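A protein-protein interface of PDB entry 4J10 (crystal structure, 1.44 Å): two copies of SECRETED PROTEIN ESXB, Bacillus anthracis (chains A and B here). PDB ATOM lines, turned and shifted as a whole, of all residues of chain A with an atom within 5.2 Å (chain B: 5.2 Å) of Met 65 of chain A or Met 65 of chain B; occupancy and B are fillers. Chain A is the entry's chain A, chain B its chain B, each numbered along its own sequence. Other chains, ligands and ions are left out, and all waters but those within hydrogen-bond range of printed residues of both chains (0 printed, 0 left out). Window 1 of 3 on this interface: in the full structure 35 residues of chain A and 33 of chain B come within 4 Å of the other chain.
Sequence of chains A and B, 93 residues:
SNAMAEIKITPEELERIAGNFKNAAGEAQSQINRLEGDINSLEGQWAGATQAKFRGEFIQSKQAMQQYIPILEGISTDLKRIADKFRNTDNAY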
ATOM      1  N   ALA A  28      26.543  -4.991  23.859  1.00  0.00           N
ATOM      2  CA  ALA A  28      25.705  -6.112  23.447  1.00  0.00           C
ATOM      3  C   ALA A  28      24.367  -6.065  24.178  1.00  0.00           C
ATOM      4  O   ALA A  28      23.313  -6.314  23.588  1.00  0.00           O
ATOM      5  CB  ALA A  28      26.418  -7.431  23.732  1.00  0.00           C
ATOM      6  N   GLN A  29      24.408  -5.776  25.476  1.00  0.00           N
ATOM      7  CA  GLN A  29      23.178  -5.612  26.252  1.00  0.00           C
ATOM      8  C   GLN A  29      22.305  -4.498  25.684  1.00  0.00           C
ATOM      9  O   GLN A  29      21.084  -4.656  25.554  1.00  0.00           O
ATOM     10  CB  GLN A  29      23.498  -5.344  27.725  1.00  0.00           C
ATOM     11  CG  GLN A  29      22.250  -5.169  28.576  1.00  0.00           C
ATOM     12  CD  GLN A  29      21.479  -6.467  28.756  1.00  0.00           C
ATOM     13  OE1 GLN A  29      20.398  -6.667  28.160  1.00  0.00           O
ATOM     14  NE2 GLN A  29      22.014  -7.350  29.573  1.00  0.00           N
ATOM     15  N   ILE A  32      20.605  -5.744  22.352  1.00  0.00           N
ATOM     16  CA  ILE A  32      19.486  -6.657  22.516  1.00  0.00           C
ATOM     17  C   ILE A  32      18.287  -5.908  23.102  1.00  0.00           C
ATOM     18  O   ILE A  32      17.144  -6.187  22.733  1.00  0.00           O
ATOM     19  CB  ILE A  32      19.898  -7.931  23.306  1.00  0.00           C
ATOM     20  CG1 ILE A  32      18.925  -9.082  23.024  1.00  0.00           C
ATOM     21  CG2 ILE A  32      20.056  -7.635  24.777  1.00  0.00           C
ATOM     22  CD1 ILE A  32      18.970  -9.533  21.577  1.00  0.00           C
ATOM     23  N   SER A  61      17.416 -15.290  19.505  1.00  0.00           N
ATOM     24  CA  SER A  61      18.583 -14.415  19.444  1.00  0.00           C
ATOM     25  C   SER A  61      18.965 -13.942  20.849  1.00  0.00           C
ATOM     26  O   SER A  61      20.143 -13.849  21.185  1.00  0.00           O
ATOM     27  CB  SER A  61      18.345 -13.236  18.487  1.00  0.00           C
ATOM     28  OG  SER A  61      17.638 -12.164  19.098  1.00  0.00           O
ATOM     29  N   LYS A  62      17.960 -13.684  21.677  1.00  0.00           N
ATOM     30  CA  LYS A  62      18.188 -13.211  23.037  1.00  0.00           C
ATOM     31  C   LYS A  62      18.870 -14.298  23.860  1.00  0.00           C
ATOM     32  O   LYS A  62      19.758 -14.013  24.667  1.00  0.00           O
ATOM     33  CB  LYS A  62      16.861 -12.761  23.672  1.00  0.00           C
ATOM     34  CG  LYS A  62      17.000 -12.095  25.044  1.00  0.00           C
ATOM     35  CD  LYS A  62      15.651 -11.581  25.519  1.00  0.00           C
ATOM     36  CE  LYS A  62      15.752 -10.856  26.843  1.00  0.00           C
ATOM     37  NZ  LYS A  62      14.400 -10.405  27.294  1.00  0.00           N
ATOM     38  N   GLN A  63      18.476 -15.550  23.649  1.00  0.00           N
ATOM     39  CA  GLN A  63      19.118 -16.662  24.338  1.00  0.00           C
ATOM     40  C   GLN A  63      20.597 -16.805  23.944  1.00  0.00           C
ATOM     41  O   GLN A  63      21.432 -17.079  24.800  1.00  0.00           O
ATOM     42  CB  GLN A  63      18.321 -17.954  24.128  1.00  0.00           C
ATOM     43  CG  GLN A  63      17.027 -17.974  24.932  1.00  0.00           C
ATOM     44  CD  GLN A  63      16.047 -19.020  24.445  1.00  0.00           C
ATOM     45  OE1 GLN A  63      16.126 -19.475  23.304  1.00  0.00           O
ATOM     46  NE2 GLN A  63      15.109 -19.399  25.305  1.00  0.00           N
ATOM     47  N   ALA A  64      20.922 -16.599  22.672  1.00  0.00           N
ATOM     48  CA  ALA A  64      22.312 -16.660  22.237  1.00  0.00           C
ATOM     49  C   ALA A  64      23.096 -15.541  22.900  1.00  0.00           C
ATOM     50  O   ALA A  64      24.234 -15.729  23.330  1.00  0.00           O
ATOM     51  CB  ALA A  64      22.412 -16.541  20.729  1.00  0.00           C
ATOM     52  N   MET A  65      22.460 -14.386  22.980  1.00  0.00           N
ATOM     53  CA  MET A  65      23.063 -13.219  23.577  1.00  0.00           C
ATOM     54  C   MET A  65      23.303 -13.404  25.075  1.00  0.00           C
ATOM     55  O   MET A  65      24.287 -12.907  25.621  1.00  0.00           O
ATOM     56  CB  MET A  65      22.169 -12.022  23.295  1.00  0.00           C
ATOM     57  CG  MET A  65      22.726 -10.716  23.729  1.00  0.00           C
ATOM     58  SD  MET A  65      24.520 -10.240  23.131  1.00  0.00           S
ATOM     59  CE  MET A  65      24.985 -11.334  21.565  1.00  0.00           C
ATOM     60  N   GLN A  66      22.409 -14.141  25.723  1.00  0.00           N
ATOM     61  CA  GLN A  66      22.518 -14.440  27.144  1.00  0.00           C
ATOM     62  C   GLN A  66      23.610 -15.457  27.455  1.00  0.00           C
ATOM     63  O   GLN A  66      23.996 -15.611  28.605  1.00  0.00           O
ATOM     64  CB  GLN A  66      21.154 -14.861  27.687  1.00  0.00           C
ATOM     65  CG  GLN A  66      20.202 -13.677  27.815  1.00  0.00           C
ATOM     66  CD  GLN A  66      18.814 -14.070  28.237  1.00  0.00           C
ATOM     67  OE1 GLN A  66      18.418 -15.224  28.100  1.00  0.00           O
ATOM     68  NE2 GLN A  66      18.057 -13.108  28.753  1.00  0.00           N
ATOM     69  N   GLN A  67      24.109 -16.138  26.427  1.00  0.00           N
ATOM     70  CA  GLN A  67      25.322 -16.942  26.550  1.00  0.00           C
ATOM     71  C   GLN A  67      26.560 -16.072  26.306  1.00  0.00           C
ATOM     72  O   GLN A  67      27.546 -16.138  27.037  1.00  0.00           O
ATOM     73  CB  GLN A  67      25.299 -18.101  25.545  1.00  0.00           C
ATOM     74  CG  GLN A  67      24.182 -19.111  25.767  1.00  0.00           C
ATOM     75  CD  GLN A  67      24.330 -19.848  27.077  1.00  0.00           C
ATOM     76  OE1 GLN A  67      25.386 -20.406  27.365  1.00  0.00           O
ATOM     77  NE2 GLN A  67      23.278 -19.844  27.882  1.00  0.00           N
ATOM     78  N   TYR A  68      26.502 -15.239  25.276  1.00  0.00           N
ATOM     79  CA  TYR A  68      27.633 -14.439  24.837  1.00  0.00           C
ATOM     80  C   TYR A  68      28.130 -13.465  25.894  1.00  0.00           C
ATOM     81  O   TYR A  68      29.326 -13.395  26.186  1.00  0.00           O
ATOM     82  CB  TYR A  68      27.196 -13.645  23.612  1.00  0.00           C
ATOM     83  CG  TYR A  68      28.240 -12.743  23.006  1.00  0.00           C
ATOM     84  CD1 TYR A  68      29.322 -13.264  22.315  1.00  0.00           C
ATOM     85  CD2 TYR A  68      28.118 -11.363  23.062  1.00  0.00           C
ATOM     86  CE1 TYR A  68      30.259 -12.446  21.739  1.00  0.00           C
ATOM     87  CE2 TYR A  68      29.049 -10.530  22.465  1.00  0.00           C
ATOM     88  CZ  TYR A  68      30.122 -11.076  21.799  1.00  0.00           C
ATOM     89  OH  TYR A  68      31.036 -10.241  21.204  1.00  0.00           O
ATOM     90  N   ILE A  69      27.202 -12.704  26.457  1.00  0.00           N
ATOM     91  CA  ILE A  69      27.541 -11.643  27.389  1.00  0.00           C
ATOM     92  C   ILE A  69      28.341 -12.158  28.596  1.00  0.00           C
ATOM     93  O   ILE A  69      29.424 -11.616  28.875  1.00  0.00           O
ATOM     94  CB  ILE A  69      26.288 -10.811  27.773  1.00  0.00           C
ATOM     95  CG1 ILE A  69      25.831  -9.988  26.565  1.00  0.00           C
ATOM     96  CG2 ILE A  69      26.572  -9.899  28.951  1.00  0.00           C
ATOM     97  CD1 ILE A  69      24.519  -9.270  26.794  1.00  0.00           C
ATOM     98  N   PRO A  70      27.861 -13.220  29.288  1.00  0.00           N
ATOM     99  CA  PRO A  70      28.681 -13.727  30.410  1.00  0.00           C
ATOM    100  C   PRO A  70      30.029 -14.306  29.997  1.00  0.00           C
ATOM    101  O   PRO A  70      30.966 -14.289  30.805  1.00  0.00           O
ATOM    102  CB  PRO A  70      27.812 -14.830  31.043  1.00  0.00           C
ATOM    103  CG  PRO A  70      26.428 -14.601  30.515  1.00  0.00           C
ATOM    104  CD  PRO A  70      26.531 -13.858  29.215  1.00  0.00           C
ATOM    105  N   ALA B  28      27.571  -6.535  15.524  1.00  0.00           N
ATOM    106  CA  ALA B  28      27.973  -7.686  16.325  1.00  0.00           C
ATOM    107  C   ALA B  28      29.198  -8.360  15.691  1.00  0.00           C
ATOM    108  O   ALA B  28      30.158  -8.716  16.395  1.00  0.00           O
ATOM    109  CB  ALA B  28      26.806  -8.642  16.420  1.00  0.00           C
ATOM    110  N   GLN B  29      29.201  -8.502  14.370  1.00  0.00           N
ATOM    111  CA  GLN B  29      30.350  -9.102  13.699  1.00  0.00           C
ATOM    112  C   GLN B  29      31.591  -8.228  13.863  1.00  0.00           C
ATOM    113  O   GLN B  29      32.694  -8.725  14.121  1.00  0.00           O
ATOM    114  CB  GLN B  29      30.067  -9.324  12.216  1.00  0.00           C
ATOM    115  CG  GLN B  29      31.222  -9.988  11.493  1.00  0.00           C
ATOM    116  CD  GLN B  29      31.480 -11.396  11.997  1.00  0.00           C
ATOM    117  OE1 GLN B  29      30.613 -12.265  11.893  1.00  0.00           O
ATOM    118  NE2 GLN B  29      32.671 -11.630  12.555  1.00  0.00           N
ATOM    119  N   ILE B  32      33.054  -8.636  17.485  1.00  0.00           N
ATOM    120  CA  ILE B  32      33.830  -9.837  17.722  1.00  0.00           C
ATOM    121  C   ILE B  32      35.156  -9.786  16.946  1.00  0.00           C
ATOM    122  O   ILE B  32      36.179 -10.275  17.426  1.00  0.00           O
ATOM    123  CB  ILE B  32      32.990 -11.120  17.483  1.00  0.00           C
ATOM    124  CG1 ILE B  32      33.567 -12.291  18.286  1.00  0.00           C
ATOM    125  CG2 ILE B  32      32.872 -11.432  16.011  1.00  0.00           C
ATOM    126  CD1 ILE B  32      32.519 -13.194  18.854  1.00  0.00           C
ATOM    127  N   SER B  61      32.683 -17.564  22.716  1.00  0.00           N
ATOM    128  CA  SER B  61      31.941 -16.348  22.398  1.00  0.00           C
ATOM    129  C   SER B  61      31.640 -16.278  20.902  1.00  0.00           C
ATOM    130  O   SER B  61      30.549 -15.853  20.507  1.00  0.00           O
ATOM    131  CB  SER B  61      32.692 -15.093  22.864  1.00  0.00           C
ATOM    132  OG  SER B  61      33.665 -14.668  21.924  1.00  0.00           O
ATOM    133  N   LYS B  62      32.585 -16.715  20.073  1.00  0.00           N
ATOM    134  CA  LYS B  62      32.378 -16.723  18.619  1.00  0.00           C
ATOM    135  C   LYS B  62      31.261 -17.673  18.231  1.00  0.00           C
ATOM    136  O   LYS B  62      30.460 -17.379  17.339  1.00  0.00           O
ATOM    137  CB  LYS B  62      33.654 -17.126  17.879  1.00  0.00           C
ATOM    138  CG  LYS B  62      34.754 -16.084  17.907  1.00  0.00           C
ATOM    139  CD  LYS B  62      35.963 -16.529  17.082  1.00  0.00           C
ATOM    140  CE  LYS B  62      35.611 -16.648  15.606  1.00  0.00           C
ATOM    141  NZ  LYS B  62      36.823 -16.814  14.763  1.00  0.00           N
ATOM    142  N   GLN B  63      31.205 -18.819  18.895  1.00  0.00           N
ATOM    143  CA  GLN B  63      30.166 -19.806  18.614  1.00  0.00           C
ATOM    144  C   GLN B  63      28.786 -19.253  18.941  1.00  0.00           C
ATOM    145  O   GLN B  63      27.834 -19.467  18.190  1.00  0.00           O
ATOM    146  CB  GLN B  63      30.438 -21.105  19.373  1.00  0.00           C
ATOM    147  CG  GLN B  63      31.676 -21.828  18.854  1.00  0.00           C
ATOM    148  CD  GLN B  63      32.075 -23.021  19.699  1.00  0.00           C
ATOM    149  OE1 GLN B  63      31.696 -23.134  20.865  1.00  0.00           O
ATOM    150  NE2 GLN B  63      32.853 -23.918  19.110  1.00  0.00           N
ATOM    151  N   ALA B  64      28.683 -18.519  20.045  1.00  0.00           N
ATOM    152  CA  ALA B  64      27.427 -17.858  20.387  1.00  0.00           C
ATOM    153  C   ALA B  64      27.027 -16.847  19.323  1.00  0.00           C
ATOM    154  O   ALA B  64      25.860 -16.749  18.950  1.00  0.00           O
ATOM    155  CB  ALA B  64      27.512 -17.197  21.754  1.00  0.00           C
ATOM    156  N   MET B  65      28.002 -16.128  18.799  1.00  0.00           N
ATOM    157  CA  MET B  65      27.701 -15.125  17.805  1.00  0.00           C
ATOM    158  C   MET B  65      27.377 -15.736  16.458  1.00  0.00           C
ATOM    159  O   MET B  65      26.648 -15.150  15.657  1.00  0.00           O
ATOM    160  CB  MET B  65      28.861 -14.160  17.716  1.00  0.00           C
ATOM    161  CG  MET B  65      28.982 -13.399  18.992  1.00  0.00           C
ATOM    162  SD  MET B  65      27.475 -12.214  19.151  1.00  0.00           S
ATOM    163  CE  MET B  65      27.587 -11.721  17.303  1.00  0.00           C
ATOM    164  N   GLN B  66      27.903 -16.930  16.221  1.00  0.00           N
ATOM    165  CA  GLN B  66      27.594 -17.670  15.001  1.00  0.00           C
ATOM    166  C   GLN B  66      26.154 -18.198  14.993  1.00  0.00           C
ATOM    167  O   GLN B  66      25.612 -18.529  13.936  1.00  0.00           O
ATOM    168  CB  GLN B  66      28.641 -18.763  14.747  1.00  0.00           C
ATOM    169  CG  GLN B  66      29.970 -18.186  14.251  1.00  0.00           C
ATOM    170  CD  GLN B  66      31.150 -19.122  14.437  1.00  0.00           C
ATOM    171  OE1 GLN B  66      30.995 -20.263  14.874  1.00  0.00           O
ATOM    172  NE2 GLN B  66      32.344 -18.635  14.112  1.00  0.00           N
ATOM    173  N   GLN B  67      25.521 -18.245  16.165  1.00  0.00           N
ATOM    174  CA  GLN B  67      24.086 -18.521  16.241  1.00  0.00           C
ATOM    175  C   GLN B  67      23.285 -17.228  16.099  1.00  0.00           C
ATOM    176  O   GLN B  67      22.318 -17.157  15.340  1.00  0.00           O
ATOM    177  CB  GLN B  67      23.731 -19.179  17.576  1.00  0.00           C
ATOM    178  CG  GLN B  67      24.341 -20.545  17.774  1.00  0.00           C
ATOM    179  CD  GLN B  67      23.796 -21.560  16.796  1.00  0.00           C
ATOM    180  OE1 GLN B  67      22.582 -21.757  16.695  1.00  0.00           O
ATOM    181  NE2 GLN B  67      24.690 -22.205  16.057  1.00  0.00           N
ATOM    182  N   TYR B  68      23.715 -16.201  16.824  1.00  0.00           N
ATOM    183  CA  TYR B  68      23.020 -14.924  16.929  1.00  0.00           C
ATOM    184  C   TYR B  68      22.857 -14.208  15.598  1.00  0.00           C
ATOM    185  O   TYR B  68      21.750 -13.792  15.224  1.00  0.00           O
ATOM    186  CB  TYR B  68      23.812 -14.027  17.878  1.00  0.00           C
ATOM    187  CG  TYR B  68      23.234 -12.652  18.150  1.00  0.00           C
ATOM    188  CD1 TYR B  68      22.066 -12.508  18.892  1.00  0.00           C
ATOM    189  CD2 TYR B  68      23.871 -11.499  17.702  1.00  0.00           C
ATOM    190  CE1 TYR B  68      21.542 -11.250  19.169  1.00  0.00           C
ATOM    191  CE2 TYR B  68      23.352 -10.228  17.986  1.00  0.00           C
ATOM    192  CZ  TYR B  68      22.192 -10.121  18.718  1.00  0.00           C
ATOM    193  OH  TYR B  68      21.681  -8.884  19.031  1.00  0.00           O
ATOM    194  N   ILE B  69      23.962 -14.051  14.880  1.00  0.00           N
ATOM    195  CA  ILE B  69      23.959 -13.284  13.639  1.00  0.00           C
ATOM    196  C   ILE B  69      22.973 -13.829  12.597  1.00  0.00           C
ATOM    197  O   ILE B  69      22.165 -13.056  12.074  1.00  0.00           O
ATOM    198  CB  ILE B  69      25.391 -13.102  13.082  1.00  0.00           C
ATOM    199  CG1 ILE B  69      26.168 -12.167  14.011  1.00  0.00           C
ATOM    200  CG2 ILE B  69      25.364 -12.544  11.656  1.00  0.00           C
ATOM    201  CD1 ILE B  69      27.659 -12.058  13.697  1.00  0.00           C
ATOM    202  N   PRO B  70      22.999 -15.146  12.302  1.00  0.00           N
ATOM    203  CA  PRO B  70      22.010 -15.621  11.314  1.00  0.00           C
ATOM    204  C   PRO B  70      20.564 -15.460  11.769  1.00  0.00           C
ATOM    205  O   PRO B  70      19.690 -15.295  10.916  1.00  0.00           O
ATOM    206  CB  PRO B  70      22.330 -17.107  11.153  1.00  0.00           C
ATOM    207  CG  PRO B  70      23.728 -17.262  11.654  1.00  0.00           C
ATOM    208  CD  PRO B  70      23.956 -16.201  12.682  1.00  0.00           C
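Of the printed residues of chain B, Met 65 of chain A touches Met 65. Of the printed residues of chain A, Met 65 of chain B touches Met 65 and Tyr 68. Of the printed residues of chain A, Tyr 68 of chain B touches Ile 32 and Ser 61. Of the printed residues of chain B, Ala 64 of chain A touches Ala 64 (3.9 Å).
Of the 13 printed residues of chain A, 5 touch a printed residue of chain B. Hydrophobic or aromatic side chains of chain A within 4 Å of the printed part of chain B: Ile 32, Ala 64, Met 65 and Tyr 68. Among the printed residues, 7 pairs touch across the chains.
Among the printed residues, merely in contact across the chains: Ile 32 of chain A with Tyr 68 of chain B (3.8 Å), Ser 61 of chain A with Tyr 68 of chain B (3.3 Å), Ala 64 of chain A with Ala 64 of chain B (3.9 Å), Met 65 of chain A with Met 65 of chain B (3.6 Å), Tyr 68 of chain A with Ile 32 of chain B (3.7 Å), Tyr 68 of chain A with Ser 61 of chain B (3.4 Å) and Tyr 68 of chain A with Met 65 of chain B (3.2 Å).
Ile 32 of chain A touches Tyr 68 of chain B, and with the chains exchanged Tyr 68 of chain A touches Ile 32 of chain B. Ala 64 of chain A touches its own counterpart, Ala 64 of chain B. Met 65 of chain B touches its own counterpart, Met 65 of chain A. Tyr 68 of chain A touches Met 65 of chain B, but with the chains exchanged Met 65 of chain A does not touch Tyr 68 of chain B (4.02 Å). Of the 7 pairs that touch across the chains among the printed residues, 6 have their exchanged pair printed and touching as well.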
